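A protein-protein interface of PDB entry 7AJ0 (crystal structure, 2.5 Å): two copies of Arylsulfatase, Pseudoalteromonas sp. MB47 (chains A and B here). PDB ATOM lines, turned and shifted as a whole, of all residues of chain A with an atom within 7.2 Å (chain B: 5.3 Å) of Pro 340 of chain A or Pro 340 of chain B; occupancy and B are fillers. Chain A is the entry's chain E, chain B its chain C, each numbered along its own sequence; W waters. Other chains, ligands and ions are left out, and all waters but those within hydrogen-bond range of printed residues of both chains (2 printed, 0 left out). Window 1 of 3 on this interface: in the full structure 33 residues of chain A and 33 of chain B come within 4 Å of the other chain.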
ATOM      1  N   GLY A  63      13.604  15.529  17.570  1.00  0.00           N
ATOM      2  CA  GLY A  63      12.734  14.788  16.688  1.00  0.00           C
ATOM      3  C   GLY A  63      12.952  13.291  16.763  1.00  0.00           C
ATOM      4  O   GLY A  63      14.017  12.805  17.139  1.00  0.00           O
ATOM      5  N   TRP A  64      11.901  12.558  16.388  1.00  0.00           N
ATOM      6  CA  TRP A  64      11.957  11.099  16.371  1.00  0.00           C
ATOM      7  C   TRP A  64      13.208  10.596  15.667  1.00  0.00           C
ATOM      8  O   TRP A  64      13.853   9.649  16.130  1.00  0.00           O
ATOM      9  CB  TRP A  64      10.700  10.558  15.680  1.00  0.00           C
ATOM     10  CG  TRP A  64      10.424   9.091  15.858  1.00  0.00           C
ATOM     11  CD1 TRP A  64       9.670   8.517  16.838  1.00  0.00           C
ATOM     12  CD2 TRP A  64      10.865   8.019  15.013  1.00  0.00           C
ATOM     13  NE1 TRP A  64       9.624   7.155  16.664  1.00  0.00           N
ATOM     14  CE2 TRP A  64      10.350   6.823  15.551  1.00  0.00           C
ATOM     15  CE3 TRP A  64      11.648   7.953  13.858  1.00  0.00           C
ATOM     16  CZ2 TRP A  64      10.597   5.577  14.978  1.00  0.00           C
ATOM     17  CZ3 TRP A  64      11.892   6.713  13.288  1.00  0.00           C
ATOM     18  CH2 TRP A  64      11.370   5.543  13.850  1.00  0.00           C
ATOM     19  N   GLY A  65      13.575  11.224  14.557  1.00  0.00           N
ATOM     20  CA  GLY A  65      14.636  10.733  13.709  1.00  0.00           C
ATOM     21  C   GLY A  65      16.014  11.299  13.960  1.00  0.00           C
ATOM     22  O   GLY A  65      16.915  11.046  13.156  1.00  0.00           O
ATOM     23  N   ASP A  66      16.220  12.046  15.049  1.00  0.00           N
ATOM     24  CA  ASP A  66      17.532  12.651  15.267  1.00  0.00           C
ATOM     25  C   ASP A  66      18.586  11.622  15.653  1.00  0.00           C
ATOM     26  O   ASP A  66      19.696  11.665  15.092  1.00  0.00           O
ATOM     27  CB  ASP A  66      17.424  13.764  16.315  1.00  0.00           C
ATOM     28  CG  ASP A  66      17.012  15.099  15.711  1.00  0.00           C
ATOM     29  OD1 ASP A  66      17.591  15.487  14.674  1.00  0.00           O
ATOM     30  OD2 ASP A  66      16.108  15.757  16.270  1.00  0.00           O
ATOM     31  N   TYR A  70      17.508   5.799  15.206  1.00  0.00           N
ATOM     32  CA  TYR A  70      16.203   6.101  14.639  1.00  0.00           C
ATOM     33  C   TYR A  70      16.279   6.533  13.178  1.00  0.00           C
ATOM     34  O   TYR A  70      15.272   6.985  12.624  1.00  0.00           O
ATOM     35  CB  TYR A  70      15.507   7.199  15.451  1.00  0.00           C
ATOM     36  CG  TYR A  70      14.901   6.744  16.761  1.00  0.00           C
ATOM     37  CD1 TYR A  70      13.616   6.220  16.809  1.00  0.00           C
ATOM     38  CD2 TYR A  70      15.604   6.860  17.952  1.00  0.00           C
ATOM     39  CE1 TYR A  70      13.055   5.813  18.004  1.00  0.00           C
ATOM     40  CE2 TYR A  70      15.053   6.453  19.152  1.00  0.00           C
ATOM     41  CZ  TYR A  70      13.779   5.932  19.175  1.00  0.00           C
ATOM     42  OH  TYR A  70      13.229   5.532  20.372  1.00  0.00           O
ATOM     43  N   GLY A  71      17.442   6.414  12.548  1.00  0.00           N
ATOM     44  CA  GLY A  71      17.600   6.800  11.164  1.00  0.00           C
ATOM     45  C   GLY A  71      18.247   8.144  10.922  1.00  0.00           C
ATOM     46  O   GLY A  71      18.316   8.574   9.765  1.00  0.00           O
ATOM     47  N   PRO A 328      10.245  18.161  16.488  1.00  0.00           N
ATOM     48  CA  PRO A 328      11.187  19.216  16.091  1.00  0.00           C
ATOM     49  C   PRO A 328      10.489  20.542  15.838  1.00  0.00           C
ATOM     50  O   PRO A 328       9.366  20.593  15.331  1.00  0.00           O
ATOM     51  CB  PRO A 328      11.820  18.662  14.808  1.00  0.00           C
ATOM     52  CG  PRO A 328      10.773  17.751  14.244  1.00  0.00           C
ATOM     53  CD  PRO A 328      10.078  17.136  15.439  1.00  0.00           C
ATOM     54  N   TYR A 338      15.362  17.083  13.487  1.00  0.00           N
ATOM     55  CA  TYR A 338      14.854  16.348  12.340  1.00  0.00           C
ATOM     56  C   TYR A 338      13.887  15.258  12.778  1.00  0.00           C
ATOM     57  O   TYR A 338      14.099  14.596  13.797  1.00  0.00           O
ATOM     58  CB  TYR A 338      16.005  15.712  11.546  1.00  0.00           C
ATOM     59  CG  TYR A 338      15.558  14.556  10.686  1.00  0.00           C
ATOM     60  CD1 TYR A 338      14.782  14.771   9.556  1.00  0.00           C
ATOM     61  CD2 TYR A 338      15.903  13.250  11.007  1.00  0.00           C
ATOM     62  CE1 TYR A 338      14.365  13.718   8.770  1.00  0.00           C
ATOM     63  CE2 TYR A 338      15.492  12.191  10.227  1.00  0.00           C
ATOM     64  CZ  TYR A 338      14.722  12.431   9.109  1.00  0.00           C
ATOM     65  OH  TYR A 338      14.310  11.379   8.326  1.00  0.00           O
ATOM     66  N   SER A 339      12.821  15.075  11.994  1.00  0.00           N
ATOM     67  CA  SER A 339      11.913  13.957  12.180  1.00  0.00           C
ATOM     68  C   SER A 339      11.388  13.526  10.819  1.00  0.00           C
ATOM     69  O   SER A 339      11.126  14.385   9.963  1.00  0.00           O
ATOM     70  CB  SER A 339      10.734  14.304  13.094  1.00  0.00           C
ATOM     71  OG  SER A 339       9.857  13.197  13.212  1.00  0.00           O
ATOM     72  N   PRO A 340      11.223  12.221  10.587  1.00  0.00           N
ATOM     73  CA  PRO A 340      10.683  11.768   9.299  1.00  0.00           C
ATOM     74  C   PRO A 340       9.190  11.987   9.147  1.00  0.00           C
ATOM     75  O   PRO A 340       8.683  11.908   8.018  1.00  0.00           O
ATOM     76  CB  PRO A 340      11.013  10.266   9.294  1.00  0.00           C
ATOM     77  CG  PRO A 340      10.992   9.892  10.739  1.00  0.00           C
ATOM     78  CD  PRO A 340      11.541  11.090  11.484  1.00  0.00           C
ATOM     79  N   TRP A 341       8.477  12.268  10.232  1.00  0.00           N
ATOM     80  CA  TRP A 341       7.029  12.318  10.188  1.00  0.00           C
ATOM     81  C   TRP A 341       6.543  13.687   9.722  1.00  0.00           C
ATOM     82  O   TRP A 341       7.314  14.639   9.578  1.00  0.00           O
ATOM     83  CB  TRP A 341       6.441  11.992  11.560  1.00  0.00           C
ATOM     84  CG  TRP A 341       7.077  10.815  12.237  1.00  0.00           C
ATOM     85  CD1 TRP A 341       7.422  10.720  13.554  1.00  0.00           C
ATOM     86  CD2 TRP A 341       7.442   9.565  11.637  1.00  0.00           C
ATOM     87  NE1 TRP A 341       7.975   9.490  13.813  1.00  0.00           N
ATOM     88  CE2 TRP A 341       7.999   8.763  12.652  1.00  0.00           C
ATOM     89  CE3 TRP A 341       7.353   9.049  10.342  1.00  0.00           C
ATOM     90  CZ2 TRP A 341       8.466   7.474  12.412  1.00  0.00           C
ATOM     91  CZ3 TRP A 341       7.820   7.769  10.106  1.00  0.00           C
ATOM     92  CH2 TRP A 341       8.366   6.995  11.136  1.00  0.00           C
ATOM     93  N   ARG A 342       5.233  13.777   9.500  1.00  0.00           N
ATOM     94  CA  ARG A 342       4.623  15.005   9.011  1.00  0.00           C
ATOM     95  C   ARG A 342       4.509  16.045  10.116  1.00  0.00           C
ATOM     96  O   ARG A 342       4.272  15.713  11.282  1.00  0.00           O
ATOM     97  CB  ARG A 342       3.237  14.710   8.439  1.00  0.00           C
ATOM     98  CG  ARG A 342       2.462  15.944   8.014  1.00  0.00           C
ATOM     99  CD  ARG A 342       1.150  15.564   7.357  1.00  0.00           C
ATOM    100  NE  ARG A 342       0.473  16.726   6.794  1.00  0.00           N
ATOM    101  CZ  ARG A 342      -0.583  16.663   5.991  1.00  0.00           C
ATOM    102  NH1 ARG A 342      -1.089  15.487   5.647  1.00  0.00           N
ATOM    103  NH2 ARG A 342      -1.131  17.776   5.529  1.00  0.00           N
ATOM    104  N   GLY A 343       4.672  17.310   9.738  1.00  0.00           N
ATOM    105  CA  GLY A 343       4.518  18.399  10.678  1.00  0.00           C
ATOM    106  C   GLY A 343       5.688  18.506  11.641  1.00  0.00           C
ATOM    107  O   GLY A 343       6.835  18.191  11.315  1.00  0.00           O
ATOM    108  N   GLY A 351       4.690  14.063  13.576  1.00  0.00           N
ATOM    109  CA  GLY A 351       5.936  14.791  13.725  1.00  0.00           C
ATOM    110  C   GLY A 351       6.011  15.622  14.983  1.00  0.00           C
ATOM    111  O   GLY A 351       7.111  15.905  15.466  1.00  0.00           O
ATOM    112  N   ARG A 354       5.201  12.116  18.109  1.00  0.00           N
ATOM    113  CA  ARG A 354       5.882  10.823  18.111  1.00  0.00           C
ATOM    114  C   ARG A 354       7.378  11.082  18.279  1.00  0.00           C
ATOM    115  O   ARG A 354       8.022  11.627  17.376  1.00  0.00           O
ATOM    116  CB  ARG A 354       5.578  10.050  16.831  1.00  0.00           C
ATOM    117  CG  ARG A 354       5.890   8.559  16.916  1.00  0.00           C
ATOM    118  CD  ARG A 354       5.454   7.829  15.650  1.00  0.00           C
ATOM    119  NE  ARG A 354       5.819   6.416  15.683  1.00  0.00           N
ATOM    120  CZ  ARG A 354       5.560   5.549  14.709  1.00  0.00           C
ATOM    121  NH1 ARG A 354       4.928   5.944  13.613  1.00  0.00           N
ATOM    122  NH2 ARG A 354       5.933   4.282  14.833  1.00  0.00           N
ATOM    123  N   PRO A 474       3.054   6.125   7.411  1.00  0.00           N
ATOM    124  CA  PRO A 474       3.640   6.751   8.608  1.00  0.00           C
ATOM    125  C   PRO A 474       3.847   8.249   8.475  1.00  0.00           C
ATOM    126  O   PRO A 474       3.917   8.941   9.498  1.00  0.00           O
ATOM    127  CB  PRO A 474       4.980   6.016   8.772  1.00  0.00           C
ATOM    128  CG  PRO A 474       5.317   5.539   7.394  1.00  0.00           C
ATOM    129  CD  PRO A 474       3.998   5.214   6.735  1.00  0.00           C
ATOM    130  N   LYS A 475       3.946   8.772   7.258  1.00  0.00           N
ATOM    131  CA  LYS A 475       4.107  10.200   7.029  1.00  0.00           C
ATOM    132  C   LYS A 475       2.775  10.914   6.831  1.00  0.00           C
ATOM    133  O   LYS A 475       2.769  12.108   6.514  1.00  0.00           O
ATOM    134  CB  LYS A 475       5.020  10.426   5.822  1.00  0.00           C
ATOM    135  CG  LYS A 475       6.434   9.894   6.037  1.00  0.00           C
ATOM    136  CD  LYS A 475       7.153   9.597   4.729  1.00  0.00           C
ATOM    137  CE  LYS A 475       7.082  10.764   3.763  1.00  0.00           C
ATOM    138  NZ  LYS A 475       7.986  10.561   2.596  1.00  0.00           N
ATOM    139  N   TRP B  64      14.703   3.926   1.535  1.00  0.00           N
ATOM    140  CA  TRP B  64      15.784   4.168   2.483  1.00  0.00           C
ATOM    141  C   TRP B  64      15.401   3.742   3.893  1.00  0.00           C
ATOM    142  O   TRP B  64      16.222   3.180   4.626  1.00  0.00           O
ATOM    143  CB  TRP B  64      16.152   5.652   2.467  1.00  0.00           C
ATOM    144  CG  TRP B  64      17.464   5.996   3.097  1.00  0.00           C
ATOM    145  CD1 TRP B  64      18.681   6.027   2.483  1.00  0.00           C
ATOM    146  CD2 TRP B  64      17.691   6.384   4.458  1.00  0.00           C
ATOM    147  NE1 TRP B  64      19.654   6.407   3.375  1.00  0.00           N
ATOM    148  CE2 TRP B  64      19.072   6.631   4.595  1.00  0.00           C
ATOM    149  CE3 TRP B  64      16.866   6.543   5.573  1.00  0.00           C
ATOM    150  CZ2 TRP B  64      19.643   7.028   5.803  1.00  0.00           C
ATOM    151  CZ3 TRP B  64      17.436   6.937   6.773  1.00  0.00           C
ATOM    152  CH2 TRP B  64      18.810   7.174   6.876  1.00  0.00           C
ATOM    153  N   GLY B  65      14.160   3.997   4.290  1.00  0.00           N
ATOM    154  CA  GLY B  65      13.723   3.780   5.650  1.00  0.00           C
ATOM    155  C   GLY B  65      13.034   2.466   5.931  1.00  0.00           C
ATOM    156  O   GLY B  65      12.475   2.306   7.022  1.00  0.00           O
ATOM    157  N   TYR B 338       8.631   2.372   2.222  1.00  0.00           N
ATOM    158  CA  TYR B 338       8.677   3.592   3.012  1.00  0.00           C
ATOM    159  C   TYR B 338      10.052   4.231   2.926  1.00  0.00           C
ATOM    160  O   TYR B 338      11.073   3.539   2.961  1.00  0.00           O
ATOM    161  CB  TYR B 338       8.335   3.304   4.482  1.00  0.00           C
ATOM    162  CG  TYR B 338       8.853   4.351   5.438  1.00  0.00           C
ATOM    163  CD1 TYR B 338       8.281   5.612   5.487  1.00  0.00           C
ATOM    164  CD2 TYR B 338       9.911   4.076   6.290  1.00  0.00           C
ATOM    165  CE1 TYR B 338       8.751   6.572   6.357  1.00  0.00           C
ATOM    166  CE2 TYR B 338      10.387   5.027   7.163  1.00  0.00           C
ATOM    167  CZ  TYR B 338       9.803   6.273   7.192  1.00  0.00           C
ATOM    168  OH  TYR B 338      10.275   7.227   8.061  1.00  0.00           O
ATOM    169  N   SER B 339      10.068   5.560   2.812  1.00  0.00           N
ATOM    170  CA  SER B 339      11.294   6.337   2.844  1.00  0.00           C
ATOM    171  C   SER B 339      10.993   7.669   3.509  1.00  0.00           C
ATOM    172  O   SER B 339       9.954   8.278   3.216  1.00  0.00           O
ATOM    173  CB  SER B 339      11.872   6.577   1.446  1.00  0.00           C
ATOM    174  OG  SER B 339      13.020   7.411   1.514  1.00  0.00           O
ATOM    175  N   PRO B 340      11.869   8.148   4.397  1.00  0.00           N
ATOM    176  CA  PRO B 340      11.638   9.467   5.008  1.00  0.00           C
ATOM    177  C   PRO B 340      11.840  10.631   4.055  1.00  0.00           C
ATOM    178  O   PRO B 340      11.395  11.742   4.365  1.00  0.00           O
ATOM    179  CB  PRO B 340      12.661   9.509   6.152  1.00  0.00           C
ATOM    180  CG  PRO B 340      13.759   8.607   5.692  1.00  0.00           C
ATOM    181  CD  PRO B 340      13.084   7.498   4.925  1.00  0.00           C
ATOM    182  N   TRP B 341      12.483  10.421   2.911  1.00  0.00           N
ATOM    183  CA  TRP B 341      12.840  11.534   2.050  1.00  0.00           C
ATOM    184  C   TRP B 341      11.668  11.933   1.155  1.00  0.00           C
ATOM    185  O   TRP B 341      10.631  11.268   1.096  1.00  0.00           O
ATOM    186  CB  TRP B 341      14.057  11.181   1.198  1.00  0.00           C
ATOM    187  CG  TRP B 341      15.151  10.509   1.964  1.00  0.00           C
ATOM    188  CD1 TRP B 341      15.907   9.453   1.548  1.00  0.00           C
ATOM    189  CD2 TRP B 341      15.610  10.836   3.282  1.00  0.00           C
ATOM    190  NE1 TRP B 341      16.810   9.104   2.523  1.00  0.00           N
ATOM    191  CE2 TRP B 341      16.646   9.937   3.598  1.00  0.00           C
ATOM    192  CE3 TRP B 341      15.244  11.800   4.224  1.00  0.00           C
ATOM    193  CZ2 TRP B 341      17.322   9.976   4.813  1.00  0.00           C
ATOM    194  CZ3 TRP B 341      15.915  11.835   5.431  1.00  0.00           C
ATOM    195  CH2 TRP B 341      16.943  10.931   5.714  1.00  0.00           C
ATOM    196  N   ARG B 342      11.851  13.042   0.449  1.00  0.00           N
ATOM    197  CA  ARG B 342      10.814  13.575  -0.418  1.00  0.00           C
ATOM    198  C   ARG B 342      10.703  12.761  -1.700  1.00  0.00           C
ATOM    199  O   ARG B 342      11.683  12.194  -2.189  1.00  0.00           O
ATOM    200  CB  ARG B 342      11.108  15.037  -0.757  1.00  0.00           C
ATOM    201  CG  ARG B 342      10.147  15.647  -1.754  1.00  0.00           C
ATOM    202  CD  ARG B 342      10.367  17.141  -1.880  1.00  0.00           C
ATOM    203  NE  ARG B 342       9.416  17.756  -2.801  1.00  0.00           N
ATOM    204  CZ  ARG B 342       9.236  19.067  -2.922  1.00  0.00           C
ATOM    205  NH1 ARG B 342       9.939  19.906  -2.173  1.00  0.00           N
ATOM    206  NH2 ARG B 342       8.350  19.539  -3.787  1.00  0.00           N
ATOM    207  N   LYS B 475      14.722  16.313   4.010  1.00  0.00           N
ATOM    208  CA  LYS B 475      13.450  16.070   3.346  1.00  0.00           C
ATOM    209  C   LYS B 475      13.171  17.069   2.231  1.00  0.00           C
ATOM    210  O   LYS B 475      12.082  17.040   1.649  1.00  0.00           O
ATOM    211  CB  LYS B 475      12.311  16.092   4.369  1.00  0.00           C
ATOM    212  CG  LYS B 475      12.473  15.059   5.471  1.00  0.00           C
ATOM    213  CD  LYS B 475      11.206  14.897   6.288  1.00  0.00           C
ATOM    214  CE  LYS B 475      10.854  16.172   7.037  1.00  0.00           C
ATOM    215  NZ  LYS B 475       9.677  15.971   7.932  1.00  0.00           N
HETATM  216  O   HOH W   1       9.097  13.269   3.796  1.00  0.00           O
HETATM  217  O   HOH W   2       7.799  18.044   8.495  1.00  0.00           O
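O of Trp 341 of chain B is in hydrogen-bond range of NZ of Lys 475 of chain A, 3.1 Å away. The side-chain amino group (NZ) of Lys 475 of chain B sits at hydrogen-bond distance from the backbone carbonyl oxygen (O) of Trp 341 of chain A (3.2 Å). O of Ser 339 of chain B lies within hydrogen-bond range of NZ of Lys 475 of chain A, 3.1 Å away. O of Ser 339 of chain A sits at hydrogen-bond distance from NZ of Lys 475 of chain B (3.0 Å).
N of Trp 341 of chain A lies close to OG of Ser 339 of chain A, 3.4 Å away. The backbone NH of Gly 65 of chain B lies within hydrogen-bond range of the backbone carbonyl oxygen of Tyr 338 of chain B, 3.4 Å away. N of Gly 65 of chain A lies within hydrogen-bond range of O of Tyr 338 of chain A. The side-chain hydroxyl (OG) of Ser 339 of chain B lies close to the backbone NH (N) of Trp 341 of chain B. The side-chain carboxylate (OD1) of Asp 66 of chain A lies within hydrogen-bond range of the backbone NH (N) of Tyr 338 of chain A (3.0 Å).
Among the printed residues, pairs that only touch across the chains: Trp 341 of chain A with Tyr 338 of chain B (3.2 Å), Gly 71 of chain A with Trp 64 of chain B (3.2 Å), Tyr 338 of chain A with Pro 340 of chain B (3.3 Å), Tyr 338 of chain A with Trp 341 of chain B (3.3 Å), Pro 340 of chain A with Tyr 338 of chain B (3.4 Å), Pro 474 of chain A with Tyr 338 of chain B (3.5 Å), Pro 340 of chain A with Pro 340 of chain B (3.6 Å) and Lys 475 of chain A with Tyr 338 of chain B (3.8 Å).
Pro 328 of chain A touches none of the printed residues of chain B. Printed residues of chain B within 4 Å of Pro 340 of chain A: Tyr 338 (3.4 Å) and Pro 340 (3.6 Å). Of the printed residues of chain A, Trp 64 of chain B touches Gly 71 (3.2 Å). Of the printed residues of chain A, Ser 339 of chain B touches Lys 475 (3.1 Å). Of the printed residues of chain A, Pro 340 of chain B touches Tyr 338 (3.3 Å) and Pro 340 (3.6 Å). Printed residues of chain A within 4 Å of Trp 341 of chain B: Tyr 338 (3.3 Å) and Lys 475 (3.1 Å). The nearest residue of chain B that does not touch Pro 340 of chain A is Lys 475 of chain B (4.2 Å). The nearest printed residue of chain A that does not touch Pro 340 of chain B is Lys 475 of chain A (4.02 Å).
Of the 17 printed residues of chain A, 7 touch a printed residue of chain B. Printed residues of chain A that touch a printed residue of chain B: Gly 71, Tyr 338, Ser 339, Pro 340, Trp 341, Pro 474 and Lys 475. Hydrophobic or aromatic side chains of chain A within 4 Å of the printed part of chain B: Tyr 338, Pro 340, Trp 341 and Pro 474. Printed residues of chain B that touch a printed residue of chain A: Trp 64, Tyr 338, Ser 339, Pro 340, Trp 341 and Lys 475. Along chain B the printed residues that touch a printed residue of chain A span positions 64 to 475. Among the printed residues, 12 pairs touch across the chains. Among the printed residues, no Asp or Glu carboxylate lies within 4 Å of a Lys or Arg side-chain nitrogen of the other chain.
Tyr 338 of chain A touches Pro 340 of chain B, and with the chains exchanged Pro 340 of chain A touches Tyr 338 of chain B. Tyr 338 of chain A touches Trp 341 of chain B, and with the chains exchanged Trp 341 of chain A touches Tyr 338 of chain B. Ser 339 of chain A touches Lys 475 of chain B, and with the chains exchanged Lys 475 of chain A touches Ser 339 of chain B. Trp 341 of chain A touches Lys 475 of chain B, and with the chains exchanged Lys 475 of chain A touches Trp 341 of chain B. Of the 12 pairs that touch across the chains among the printed residues, 9 have their exchanged pair printed and touching as well.
Water W1 lies within hydrogen-bond range of the backbone carbonyl oxygen (O) of Pro 340 of chain B (2.8 Å) and the side-chain amino group (NZ) of Lys 475 of chain A (3.2 Å). Water W2 lies within hydrogen-bond range of the side-chain amino group of Lys 475 of chain B (2.9 Å) and the backbone carbonyl oxygen of Gly 343 of chain A (3.0 Å).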
